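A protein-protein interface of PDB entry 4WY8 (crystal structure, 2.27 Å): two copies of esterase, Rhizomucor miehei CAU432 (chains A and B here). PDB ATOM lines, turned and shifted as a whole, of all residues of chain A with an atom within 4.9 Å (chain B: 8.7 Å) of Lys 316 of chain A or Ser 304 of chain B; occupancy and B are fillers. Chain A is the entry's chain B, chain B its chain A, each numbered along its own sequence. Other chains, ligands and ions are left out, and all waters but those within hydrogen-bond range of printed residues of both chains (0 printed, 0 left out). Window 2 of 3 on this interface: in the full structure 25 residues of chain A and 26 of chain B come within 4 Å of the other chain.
OE2 of Glu 305 of chain B lies within salt-bridge range of NH1 of Arg 252 of chain A, at 3.1 Å.
OD2 of Asp 308 of chain B is in salt-bridge range of NZ of Lys 316 of chain A (2.8 Å).
The side-chain carboxylate of Glu 106 of chain B lies within salt-bridge range of the guanidinium group of Arg 110 of chain B.
NH2 of Arg 110 of chain B sits at hydrogen-bond distance from OG of Ser 304 of chain B, at 2.7 Å.
The side-chain carboxylate (OD1) of Asp 308 of chain B lies within salt-bridge range of the guanidinium group (NH1) of Arg 110 of chain B, 2.7 Å away.
The guanidinium group of Arg 252 of chain A sits at hydrogen-bond distance from the side-chain hydroxyl of Thr 317 of chain A (2.9 Å).
The backbone carbonyl oxygen (O) of Trp 313 of chain A is in hydrogen-bond range of the side-chain hydroxyl (OG1) of Thr 317 of chain A, at 2.9 Å.
Among the printed residues, merely in contact across the chains: Ala 312 of chain A with Asp 308 of chain B (3.7 Å), Trp 313 of chain A with Glu 305 of chain B (3.6 Å), Lys 316 of chain A with Arg 110 of chain B (3.6 Å) and Lys 316 of chain A with Ser 304 of chain B (3.6 Å).
Printed residues of chain B within 4 Å of Ala 312 of chain A: Asp 308.
Lys 316 of chain A touches just these residues of chain B: Arg 110 (3.6 Å), Ser 304 (3.6 Å) and Asp 308 (2.8 Å).
Phe 294 of chain B touches none of the printed residues of chain A.
Of chain A, only Lys 316 comes within 4 Å of Ser 304 of chain B.
Printed residues of chain A within 4 Å of Asp 308 of chain B: Ala 312 (3.7 Å) and Lys 316 (2.8 Å).
Hydrophobic or aromatic side chains of chain A within 4 Å of the printed part of chain B: Ala 312 and Trp 313.
No position is printed for both chains.
Of the 6 pairs that touch across the chains among the printed residues, none has its exchanged pair printed and touching as well.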
ATOM      1  N   ARG A 252      -7.714  17.466  -5.437  1.00  0.00           N
ATOM      2  CA  ARG A 252      -6.546  17.822  -4.649  1.00  0.00           C
ATOM      3  C   ARG A 252      -5.336  16.928  -4.995  1.00  0.00           C
ATOM      4  O   ARG A 252      -5.433  15.692  -5.015  1.00  0.00           O
ATOM      5  CB  ARG A 252      -6.932  17.735  -3.159  1.00  0.00           C
ATOM      6  CG  ARG A 252      -5.818  17.964  -2.157  1.00  0.00           C
ATOM      7  CD  ARG A 252      -6.347  17.916  -0.716  1.00  0.00           C
ATOM      8  NE  ARG A 252      -5.334  17.433   0.223  1.00  0.00           N
ATOM      9  CZ  ARG A 252      -4.427  18.213   0.799  1.00  0.00           C
ATOM     10  NH1 ARG A 252      -4.404  19.503   0.527  1.00  0.00           N
ATOM     11  NH2 ARG A 252      -3.537  17.700   1.632  1.00  0.00           N
ATOM     12  N   ALA A 312       1.321  11.454   5.283  1.00  0.00           N
ATOM     13  CA  ALA A 312       0.899  12.680   5.971  1.00  0.00           C
ATOM     14  C   ALA A 312      -0.078  13.497   5.116  1.00  0.00           C
ATOM     15  O   ALA A 312      -1.117  13.990   5.597  1.00  0.00           O
ATOM     16  CB  ALA A 312       2.110  13.526   6.343  1.00  0.00           C
ATOM     17  N   TRP A 313       0.251  13.618   3.836  1.00  0.00           N
ATOM     18  CA  TRP A 313      -0.612  14.325   2.915  1.00  0.00           C
ATOM     19  C   TRP A 313      -1.993  13.689   2.776  1.00  0.00           C
ATOM     20  O   TRP A 313      -3.002  14.406   2.726  1.00  0.00           O
ATOM     21  CB  TRP A 313       0.052  14.396   1.559  1.00  0.00           C
ATOM     22  CG  TRP A 313      -0.710  15.172   0.564  1.00  0.00           C
ATOM     23  CD1 TRP A 313      -0.616  16.513   0.323  1.00  0.00           C
ATOM     24  CD2 TRP A 313      -1.664  14.658  -0.376  1.00  0.00           C
ATOM     25  NE1 TRP A 313      -1.459  16.865  -0.703  1.00  0.00           N
ATOM     26  CE2 TRP A 313      -2.102  15.748  -1.158  1.00  0.00           C
ATOM     27  CE3 TRP A 313      -2.188  13.382  -0.630  1.00  0.00           C
ATOM     28  CZ2 TRP A 313      -3.055  15.604  -2.170  1.00  0.00           C
ATOM     29  CZ3 TRP A 313      -3.136  13.238  -1.631  1.00  0.00           C
ATOM     30  CH2 TRP A 313      -3.557  14.347  -2.391  1.00  0.00           C
ATOM     31  N   LEU A 314      -2.033  12.357   2.711  1.00  0.00           N
ATOM     32  CA  LEU A 314      -3.281  11.605   2.645  1.00  0.00           C
ATOM     33  C   LEU A 314      -4.133  11.814   3.884  1.00  0.00           C
ATOM     34  O   LEU A 314      -5.364  11.945   3.794  1.00  0.00           O
ATOM     35  CB  LEU A 314      -3.006  10.110   2.494  1.00  0.00           C
ATOM     36  CG  LEU A 314      -2.453   9.559   1.186  1.00  0.00           C
ATOM     37  CD1 LEU A 314      -2.051   8.088   1.365  1.00  0.00           C
ATOM     38  CD2 LEU A 314      -3.493   9.704   0.103  1.00  0.00           C
ATOM     39  N   GLN A 315      -3.492  11.797   5.048  1.00  0.00           N
ATOM     40  CA  GLN A 315      -4.231  12.015   6.278  1.00  0.00           C
ATOM     41  C   GLN A 315      -4.831  13.412   6.267  1.00  0.00           C
ATOM     42  O   GLN A 315      -5.991  13.585   6.635  1.00  0.00           O
ATOM     43  CB  GLN A 315      -3.339  11.808   7.501  1.00  0.00           C
ATOM     44  CG  GLN A 315      -3.157  10.318   7.824  1.00  0.00           C
ATOM     45  CD  GLN A 315      -1.954  10.020   8.710  1.00  0.00           C
ATOM     46  OE1 GLN A 315      -1.108  10.888   8.950  1.00  0.00           O
ATOM     47  NE2 GLN A 315      -1.863   8.779   9.182  1.00  0.00           N
ATOM     48  N   LYS A 316      -4.077  14.409   5.807  1.00  0.00           N
ATOM     49  CA  LYS A 316      -4.673  15.745   5.709  1.00  0.00           C
ATOM     50  C   LYS A 316      -5.870  15.720   4.740  1.00  0.00           C
ATOM     51  O   LYS A 316      -6.937  16.250   5.052  1.00  0.00           O
ATOM     52  CB  LYS A 316      -3.632  16.781   5.297  1.00  0.00           C
ATOM     53  CG  LYS A 316      -4.161  18.214   5.056  1.00  0.00           C
ATOM     54  CD  LYS A 316      -5.021  18.731   6.211  1.00  0.00           C
ATOM     55  CE  LYS A 316      -4.256  18.882   7.522  1.00  0.00           C
ATOM     56  NZ  LYS A 316      -3.397  20.116   7.556  1.00  0.00           N
ATOM     57  N   THR A 317      -5.706  15.080   3.586  1.00  0.00           N
ATOM     58  CA  THR A 317      -6.803  14.942   2.617  1.00  0.00           C
ATOM     59  C   THR A 317      -8.091  14.358   3.238  1.00  0.00           C
ATOM     60  O   THR A 317      -9.192  14.913   3.094  1.00  0.00           O
ATOM     61  CB  THR A 317      -6.365  14.062   1.435  1.00  0.00           C
ATOM     62  OG1 THR A 317      -5.203  14.636   0.817  1.00  0.00           O
ATOM     63  CG2 THR A 317      -7.468  13.963   0.415  1.00  0.00           C
ATOM     64  N   TRP A 318      -7.931  13.251   3.953  1.00  0.00           N
ATOM     65  CA  TRP A 318      -9.038  12.571   4.592  1.00  0.00           C
ATOM     66  C   TRP A 318      -9.673  13.423   5.675  1.00  0.00           C
ATOM     67  O   TRP A 318     -10.891  13.369   5.865  1.00  0.00           O
ATOM     68  CB  TRP A 318      -8.564  11.234   5.149  1.00  0.00           C
ATOM     69  CG  TRP A 318      -8.160  10.304   4.035  1.00  0.00           C
ATOM     70  CD1 TRP A 318      -8.669  10.294   2.771  1.00  0.00           C
ATOM     71  CD2 TRP A 318      -7.150   9.275   4.068  1.00  0.00           C
ATOM     72  NE1 TRP A 318      -8.062   9.322   2.019  1.00  0.00           N
ATOM     73  CE2 TRP A 318      -7.124   8.684   2.787  1.00  0.00           C
ATOM     74  CE3 TRP A 318      -6.290   8.790   5.055  1.00  0.00           C
ATOM     75  CZ2 TRP A 318      -6.255   7.616   2.468  1.00  0.00           C
ATOM     76  CZ3 TRP A 318      -5.428   7.729   4.738  1.00  0.00           C
ATOM     77  CH2 TRP A 318      -5.423   7.154   3.459  1.00  0.00           C
ATOM     78  N   LYS A 319      -8.869  14.209   6.389  1.00  0.00           N
ATOM     79  CA  LYS A 319      -9.433  15.158   7.359  1.00  0.00           C
ATOM     80  C   LYS A 319     -10.229  16.291   6.709  1.00  0.00           C
ATOM     81  O   LYS A 319     -11.279  16.675   7.203  1.00  0.00           O
ATOM     82  CB  LYS A 319      -8.326  15.772   8.227  1.00  0.00           C
ATOM     83  CG  LYS A 319      -7.822  14.854   9.324  1.00  0.00           C
ATOM     84  CD  LYS A 319      -6.710  15.521  10.131  1.00  0.00           C
ATOM     85  CE  LYS A 319      -5.912  14.476  10.928  1.00  0.00           C
ATOM     86  NZ  LYS A 319      -4.806  15.084  11.728  1.00  0.00           N
ATOM     87  N   LEU A 320      -9.706  16.843   5.615  1.00  0.00           N
ATOM     88  CA  LEU A 320     -10.395  17.914   4.900  1.00  0.00           C
ATOM     89  C   LEU A 320     -11.746  17.445   4.401  1.00  0.00           C
ATOM     90  O   LEU A 320     -12.741  18.161   4.535  1.00  0.00           O
ATOM     91  CB  LEU A 320      -9.573  18.433   3.718  1.00  0.00           C
ATOM     92  CG  LEU A 320      -8.311  19.219   4.073  1.00  0.00           C
ATOM     93  CD1 LEU A 320      -7.543  19.633   2.811  1.00  0.00           C
ATOM     94  CD2 LEU A 320      -8.635  20.421   4.946  1.00  0.00           C
ATOM     95  N   ARG B 102       2.231  31.948  14.697  1.00  0.00           N
ATOM     96  CA  ARG B 102       1.382  31.044  13.926  1.00  0.00           C
ATOM     97  C   ARG B 102       2.110  29.706  13.679  1.00  0.00           C
ATOM     98  O   ARG B 102       1.617  28.618  14.016  1.00  0.00           O
ATOM     99  CB  ARG B 102       0.981  31.730  12.608  1.00  0.00           C
ATOM    100  CG  ARG B 102       0.272  30.827  11.596  1.00  0.00           C
ATOM    101  CD  ARG B 102      -1.147  30.516  11.988  1.00  0.00           C
ATOM    102  NE  ARG B 102      -1.934  31.754  12.038  1.00  0.00           N
ATOM    103  CZ  ARG B 102      -3.245  31.807  12.258  1.00  0.00           C
ATOM    104  NH1 ARG B 102      -3.944  30.695  12.436  1.00  0.00           N
ATOM    105  NH2 ARG B 102      -3.856  32.976  12.284  1.00  0.00           N
ATOM    106  N   THR B 103       3.309  29.813  13.114  1.00  0.00           N
ATOM    107  CA  THR B 103       4.120  28.650  12.803  1.00  0.00           C
ATOM    108  C   THR B 103       4.381  27.773  14.035  1.00  0.00           C
ATOM    109  O   THR B 103       4.210  26.545  13.999  1.00  0.00           O
ATOM    110  CB  THR B 103       5.459  29.103  12.208  1.00  0.00           C
ATOM    111  OG1 THR B 103       5.208  29.844  11.000  1.00  0.00           O
ATOM    112  CG2 THR B 103       6.343  27.895  11.921  1.00  0.00           C
ATOM    113  N   GLU B 106       1.144  26.109  15.565  1.00  0.00           N
ATOM    114  CA  GLU B 106       0.749  24.972  14.699  1.00  0.00           C
ATOM    115  C   GLU B 106       1.690  23.766  14.834  1.00  0.00           C
ATOM    116  O   GLU B 106       1.253  22.627  14.914  1.00  0.00           O
ATOM    117  CB  GLU B 106       0.691  25.408  13.226  1.00  0.00           C
ATOM    118  CG  GLU B 106      -0.532  26.250  12.855  1.00  0.00           C
ATOM    119  CD  GLU B 106      -1.869  25.489  12.905  1.00  0.00           C
ATOM    120  OE1 GLU B 106      -1.885  24.231  12.888  1.00  0.00           O
ATOM    121  OE2 GLU B 106      -2.922  26.169  12.938  1.00  0.00           O
ATOM    122  N   ARG B 110       0.514  20.130  16.140  1.00  0.00           N
ATOM    123  CA  ARG B 110       0.550  19.063  15.143  1.00  0.00           C
ATOM    124  C   ARG B 110       1.574  17.997  15.533  1.00  0.00           C
ATOM    125  O   ARG B 110       1.332  16.825  15.359  1.00  0.00           O
ATOM    126  CB  ARG B 110       0.855  19.612  13.755  1.00  0.00           C
ATOM    127  CG  ARG B 110      -0.273  20.468  13.181  1.00  0.00           C
ATOM    128  CD  ARG B 110       0.061  20.905  11.763  1.00  0.00           C
ATOM    129  NE  ARG B 110      -0.702  22.078  11.337  1.00  0.00           N
ATOM    130  CZ  ARG B 110      -0.946  22.394  10.066  1.00  0.00           C
ATOM    131  NH1 ARG B 110      -0.498  21.610   9.085  1.00  0.00           N
ATOM    132  NH2 ARG B 110      -1.622  23.504   9.776  1.00  0.00           N
ATOM    133  N   TYR B 286       9.983  22.855  -2.621  1.00  0.00           N
ATOM    134  CA  TYR B 286       8.550  23.027  -2.848  1.00  0.00           C
ATOM    135  C   TYR B 286       8.311  23.989  -3.988  1.00  0.00           C
ATOM    136  O   TYR B 286       8.882  25.090  -4.010  1.00  0.00           O
ATOM    137  CB  TYR B 286       7.850  23.516  -1.584  1.00  0.00           C
ATOM    138  CG  TYR B 286       7.401  22.378  -0.683  1.00  0.00           C
ATOM    139  CD1 TYR B 286       8.319  21.672   0.098  1.00  0.00           C
ATOM    140  CD2 TYR B 286       6.058  22.026  -0.597  1.00  0.00           C
ATOM    141  CE1 TYR B 286       7.908  20.613   0.921  1.00  0.00           C
ATOM    142  CE2 TYR B 286       5.639  20.988   0.233  1.00  0.00           C
ATOM    143  CZ  TYR B 286       6.570  20.294   0.987  1.00  0.00           C
ATOM    144  OH  TYR B 286       6.146  19.279   1.806  1.00  0.00           O
ATOM    145  N   ILE B 289       6.293  28.444  -4.350  1.00  0.00           N
ATOM    146  CA  ILE B 289       6.288  29.246  -3.133  1.00  0.00           C
ATOM    147  C   ILE B 289       7.474  30.185  -3.046  1.00  0.00           C
ATOM    148  O   ILE B 289       8.500  30.010  -3.712  1.00  0.00           O
ATOM    149  CB  ILE B 289       6.276  28.374  -1.843  1.00  0.00           C
ATOM    150  CG1 ILE B 289       7.571  27.578  -1.709  1.00  0.00           C
ATOM    151  CG2 ILE B 289       5.084  27.451  -1.818  1.00  0.00           C
ATOM    152  CD1 ILE B 289       7.743  26.998  -0.341  1.00  0.00           C
ATOM    153  N   ILE B 293       7.035  32.408   4.231  1.00  0.00           N
ATOM    154  CA  ILE B 293       5.687  32.000   4.565  1.00  0.00           C
ATOM    155  C   ILE B 293       5.536  31.643   6.046  1.00  0.00           C
ATOM    156  O   ILE B 293       4.416  31.554   6.544  1.00  0.00           O
ATOM    157  CB  ILE B 293       5.218  30.847   3.668  1.00  0.00           C
ATOM    158  CG1 ILE B 293       6.144  29.640   3.741  1.00  0.00           C
ATOM    159  CG2 ILE B 293       5.163  31.336   2.217  1.00  0.00           C
ATOM    160  CD1 ILE B 293       5.701  28.541   2.769  1.00  0.00           C
ATOM    161  N   PHE B 294       6.647  31.467   6.761  1.00  0.00           N
ATOM    162  CA  PHE B 294       6.558  31.064   8.170  1.00  0.00           C
ATOM    163  C   PHE B 294       6.777  32.181   9.200  1.00  0.00           C
ATOM    164  O   PHE B 294       6.821  31.908  10.416  1.00  0.00           O
ATOM    165  CB  PHE B 294       7.541  29.919   8.444  1.00  0.00           C
ATOM    166  CG  PHE B 294       7.178  28.654   7.732  1.00  0.00           C
ATOM    167  CD1 PHE B 294       6.028  27.961   8.085  1.00  0.00           C
ATOM    168  CD2 PHE B 294       7.967  28.166   6.699  1.00  0.00           C
ATOM    169  CE1 PHE B 294       5.673  26.790   7.420  1.00  0.00           C
ATOM    170  CE2 PHE B 294       7.625  26.997   6.026  1.00  0.00           C
ATOM    171  CZ  PHE B 294       6.480  26.307   6.390  1.00  0.00           C
ATOM    172  N   THR B 298      -0.598  34.859   9.347  1.00  0.00           N
ATOM    173  CA  THR B 298      -1.342  33.689   8.880  1.00  0.00           C
ATOM    174  C   THR B 298      -0.407  32.666   8.237  1.00  0.00           C
ATOM    175  O   THR B 298       0.773  32.929   8.018  1.00  0.00           O
ATOM    176  CB  THR B 298      -2.391  34.070   7.848  1.00  0.00           C
ATOM    177  OG1 THR B 298      -1.734  34.801   6.801  1.00  0.00           O
ATOM    178  CG2 THR B 298      -3.469  34.952   8.475  1.00  0.00           C
ATOM    179  N   LEU B 299      -0.957  31.516   7.888  1.00  0.00           N
ATOM    180  CA  LEU B 299      -0.177  30.444   7.290  1.00  0.00           C
ATOM    181  C   LEU B 299      -0.774  30.024   5.962  1.00  0.00           C
ATOM    182  O   LEU B 299      -1.926  29.604   5.923  1.00  0.00           O
ATOM    183  CB  LEU B 299      -0.122  29.253   8.257  1.00  0.00           C
ATOM    184  CG  LEU B 299       0.732  28.074   7.802  1.00  0.00           C
ATOM    185  CD1 LEU B 299       2.195  28.505   7.697  1.00  0.00           C
ATOM    186  CD2 LEU B 299       0.569  26.927   8.796  1.00  0.00           C
ATOM    187  N   SER B 300       0.009  30.106   4.884  1.00  0.00           N
ATOM    188  CA  SER B 300      -0.485  29.742   3.555  1.00  0.00           C
ATOM    189  C   SER B 300      -0.857  28.260   3.520  1.00  0.00           C
ATOM    190  O   SER B 300      -0.395  27.491   4.356  1.00  0.00           O
ATOM    191  CB  SER B 300       0.556  30.046   2.470  1.00  0.00           C
ATOM    192  OG  SER B 300       1.627  29.122   2.447  1.00  0.00           O
ATOM    193  N   PRO B 301      -1.731  27.866   2.578  1.00  0.00           N
ATOM    194  CA  PRO B 301      -2.050  26.436   2.440  1.00  0.00           C
ATOM    195  C   PRO B 301      -0.784  25.562   2.276  1.00  0.00           C
ATOM    196  O   PRO B 301      -0.632  24.515   2.943  1.00  0.00           O
ATOM    197  CB  PRO B 301      -2.924  26.395   1.180  1.00  0.00           C
ATOM    198  CG  PRO B 301      -3.558  27.784   1.118  1.00  0.00           C
ATOM    199  CD  PRO B 301      -2.507  28.714   1.647  1.00  0.00           C
ATOM    200  N   THR B 302       0.137  26.002   1.421  1.00  0.00           N
ATOM    201  CA  THR B 302       1.343  25.220   1.229  1.00  0.00           C
ATOM    202  C   THR B 302       2.188  25.217   2.496  1.00  0.00           C
ATOM    203  O   THR B 302       2.833  24.211   2.806  1.00  0.00           O
ATOM    204  CB  THR B 302       2.201  25.730   0.082  1.00  0.00           C
ATOM    205  OG1 THR B 302       1.379  25.986  -1.068  1.00  0.00           O
ATOM    206  CG2 THR B 302       3.265  24.674  -0.258  1.00  0.00           C
ATOM    207  N   GLY B 303       2.190  26.328   3.236  1.00  0.00           N
ATOM    208  CA  GLY B 303       2.885  26.372   4.516  1.00  0.00           C
ATOM    209  C   GLY B 303       2.389  25.252   5.419  1.00  0.00           C
ATOM    210  O   GLY B 303       3.173  24.549   6.075  1.00  0.00           O
ATOM    211  N   SER B 304       1.075  25.067   5.434  1.00  0.00           N
ATOM    212  CA  SER B 304       0.456  24.014   6.241  1.00  0.00           C
ATOM    213  C   SER B 304       0.828  22.613   5.759  1.00  0.00           C
ATOM    214  O   SER B 304       1.080  21.691   6.584  1.00  0.00           O
ATOM    215  CB  SER B 304      -1.065  24.187   6.260  1.00  0.00           C
ATOM    216  OG  SER B 304      -1.673  23.216   7.098  1.00  0.00           O
ATOM    217  N   GLU B 305       0.841  22.427   4.439  1.00  0.00           N
ATOM    218  CA  GLU B 305       1.273  21.123   3.934  1.00  0.00           C
ATOM    219  C   GLU B 305       2.702  20.845   4.404  1.00  0.00           C
ATOM    220  O   GLU B 305       3.026  19.756   4.885  1.00  0.00           O
ATOM    221  CB  GLU B 305       1.213  21.055   2.408  1.00  0.00           C
ATOM    222  CG  GLU B 305      -0.131  21.423   1.801  1.00  0.00           C
ATOM    223  CD  GLU B 305      -1.284  20.517   2.225  1.00  0.00           C
ATOM    224  OE1 GLU B 305      -1.084  19.309   2.540  1.00  0.00           O
ATOM    225  OE2 GLU B 305      -2.421  21.044   2.258  1.00  0.00           O
ATOM    226  N   ILE B 306       3.543  21.859   4.302  1.00  0.00           N
ATOM    227  CA  ILE B 306       4.941  21.732   4.673  1.00  0.00           C
ATOM    228  C   ILE B 306       5.060  21.367   6.128  1.00  0.00           C
ATOM    229  O   ILE B 306       5.845  20.484   6.466  1.00  0.00           O
ATOM    230  CB  ILE B 306       5.727  23.024   4.376  1.00  0.00           C
ATOM    231  CG1 ILE B 306       5.956  23.176   2.874  1.00  0.00           C
ATOM    232  CG2 ILE B 306       7.090  23.050   5.084  1.00  0.00           C
ATOM    233  CD1 ILE B 306       6.490  24.602   2.508  1.00  0.00           C
ATOM    234  N   LEU B 307       4.270  21.997   6.991  1.00  0.00           N
ATOM    235  CA  LEU B 307       4.279  21.603   8.409  1.00  0.00           C
ATOM    236  C   LEU B 307       3.831  20.149   8.625  1.00  0.00           C
ATOM    237  O   LEU B 307       4.392  19.450   9.475  1.00  0.00           O
ATOM    238  CB  LEU B 307       3.407  22.541   9.242  1.00  0.00           C
ATOM    239  CG  LEU B 307       4.008  23.924   9.484  1.00  0.00           C
ATOM    240  CD1 LEU B 307       3.162  24.611  10.522  1.00  0.00           C
ATOM    241  CD2 LEU B 307       5.442  23.824   9.973  1.00  0.00           C
ATOM    242  N   ASP B 308       2.829  19.683   7.880  1.00  0.00           N
ATOM    243  CA  ASP B 308       2.434  18.276   7.997  1.00  0.00           C
ATOM    244  C   ASP B 308       3.594  17.324   7.599  1.00  0.00           C
ATOM    245  O   ASP B 308       3.825  16.274   8.222  1.00  0.00           O
ATOM    246  CB  ASP B 308       1.192  17.998   7.139  1.00  0.00           C
ATOM    247  CG  ASP B 308      -0.082  18.630   7.721  1.00  0.00           C
ATOM    248  OD1 ASP B 308      -0.107  18.946   8.944  1.00  0.00           O
ATOM    249  OD2 ASP B 308      -1.054  18.814   6.939  1.00  0.00           O
ATOM    250  N   HIS B 309       4.321  17.722   6.562  1.00  0.00           N
ATOM    251  CA  HIS B 309       5.515  17.010   6.132  1.00  0.00           C
ATOM    252  C   HIS B 309       6.600  16.956   7.209  1.00  0.00           C
ATOM    253  O   HIS B 309       7.114  15.874   7.553  1.00  0.00           O
ATOM    254  CB  HIS B 309       6.047  17.670   4.879  1.00  0.00           C
ATOM    255  CG  HIS B 309       7.211  16.965   4.282  1.00  0.00           C
ATOM    256  ND1 HIS B 309       7.842  17.416   3.147  1.00  0.00           N
ATOM    257  CD2 HIS B 309       7.847  15.826   4.650  1.00  0.00           C
ATOM    258  CE1 HIS B 309       8.820  16.578   2.833  1.00  0.00           C
ATOM    259  NE2 HIS B 309       8.846  15.613   3.731  1.00  0.00           N
ATOM    260  N   ILE B 310       6.950  18.124   7.737  1.00  0.00           N
ATOM    261  CA  ILE B 310       7.920  18.218   8.821  1.00  0.00           C
ATOM    262  C   ILE B 310       7.525  17.330   9.993  1.00  0.00           C
ATOM    263  O   ILE B 310       8.362  16.642  10.571  1.00  0.00           O
ATOM    264  CB  ILE B 310       8.060  19.679   9.316  1.00  0.00           C
ATOM    265  CG1 ILE B 310       8.774  20.531   8.254  1.00  0.00           C
ATOM    266  CG2 ILE B 310       8.837  19.762  10.627  1.00  0.00           C
ATOM    267  CD1 ILE B 310       8.717  22.007   8.552  1.00  0.00           C
ATOM    268  N   VAL B 311       6.243  17.338  10.335  1.00  0.00           N
ATOM    269  CA  VAL B 311       5.776  16.524  11.436  1.00  0.00           C
ATOM    270  C   VAL B 311       5.917  15.036  11.131  1.00  0.00           C
ATOM    271  O   VAL B 311       6.353  14.273  11.998  1.00  0.00           O
ATOM    272  CB  VAL B 311       4.317  16.858  11.775  1.00  0.00           C
ATOM    273  CG1 VAL B 311       3.741  15.830  12.781  1.00  0.00           C
ATOM    274  CG2 VAL B 311       4.247  18.267  12.325  1.00  0.00           C
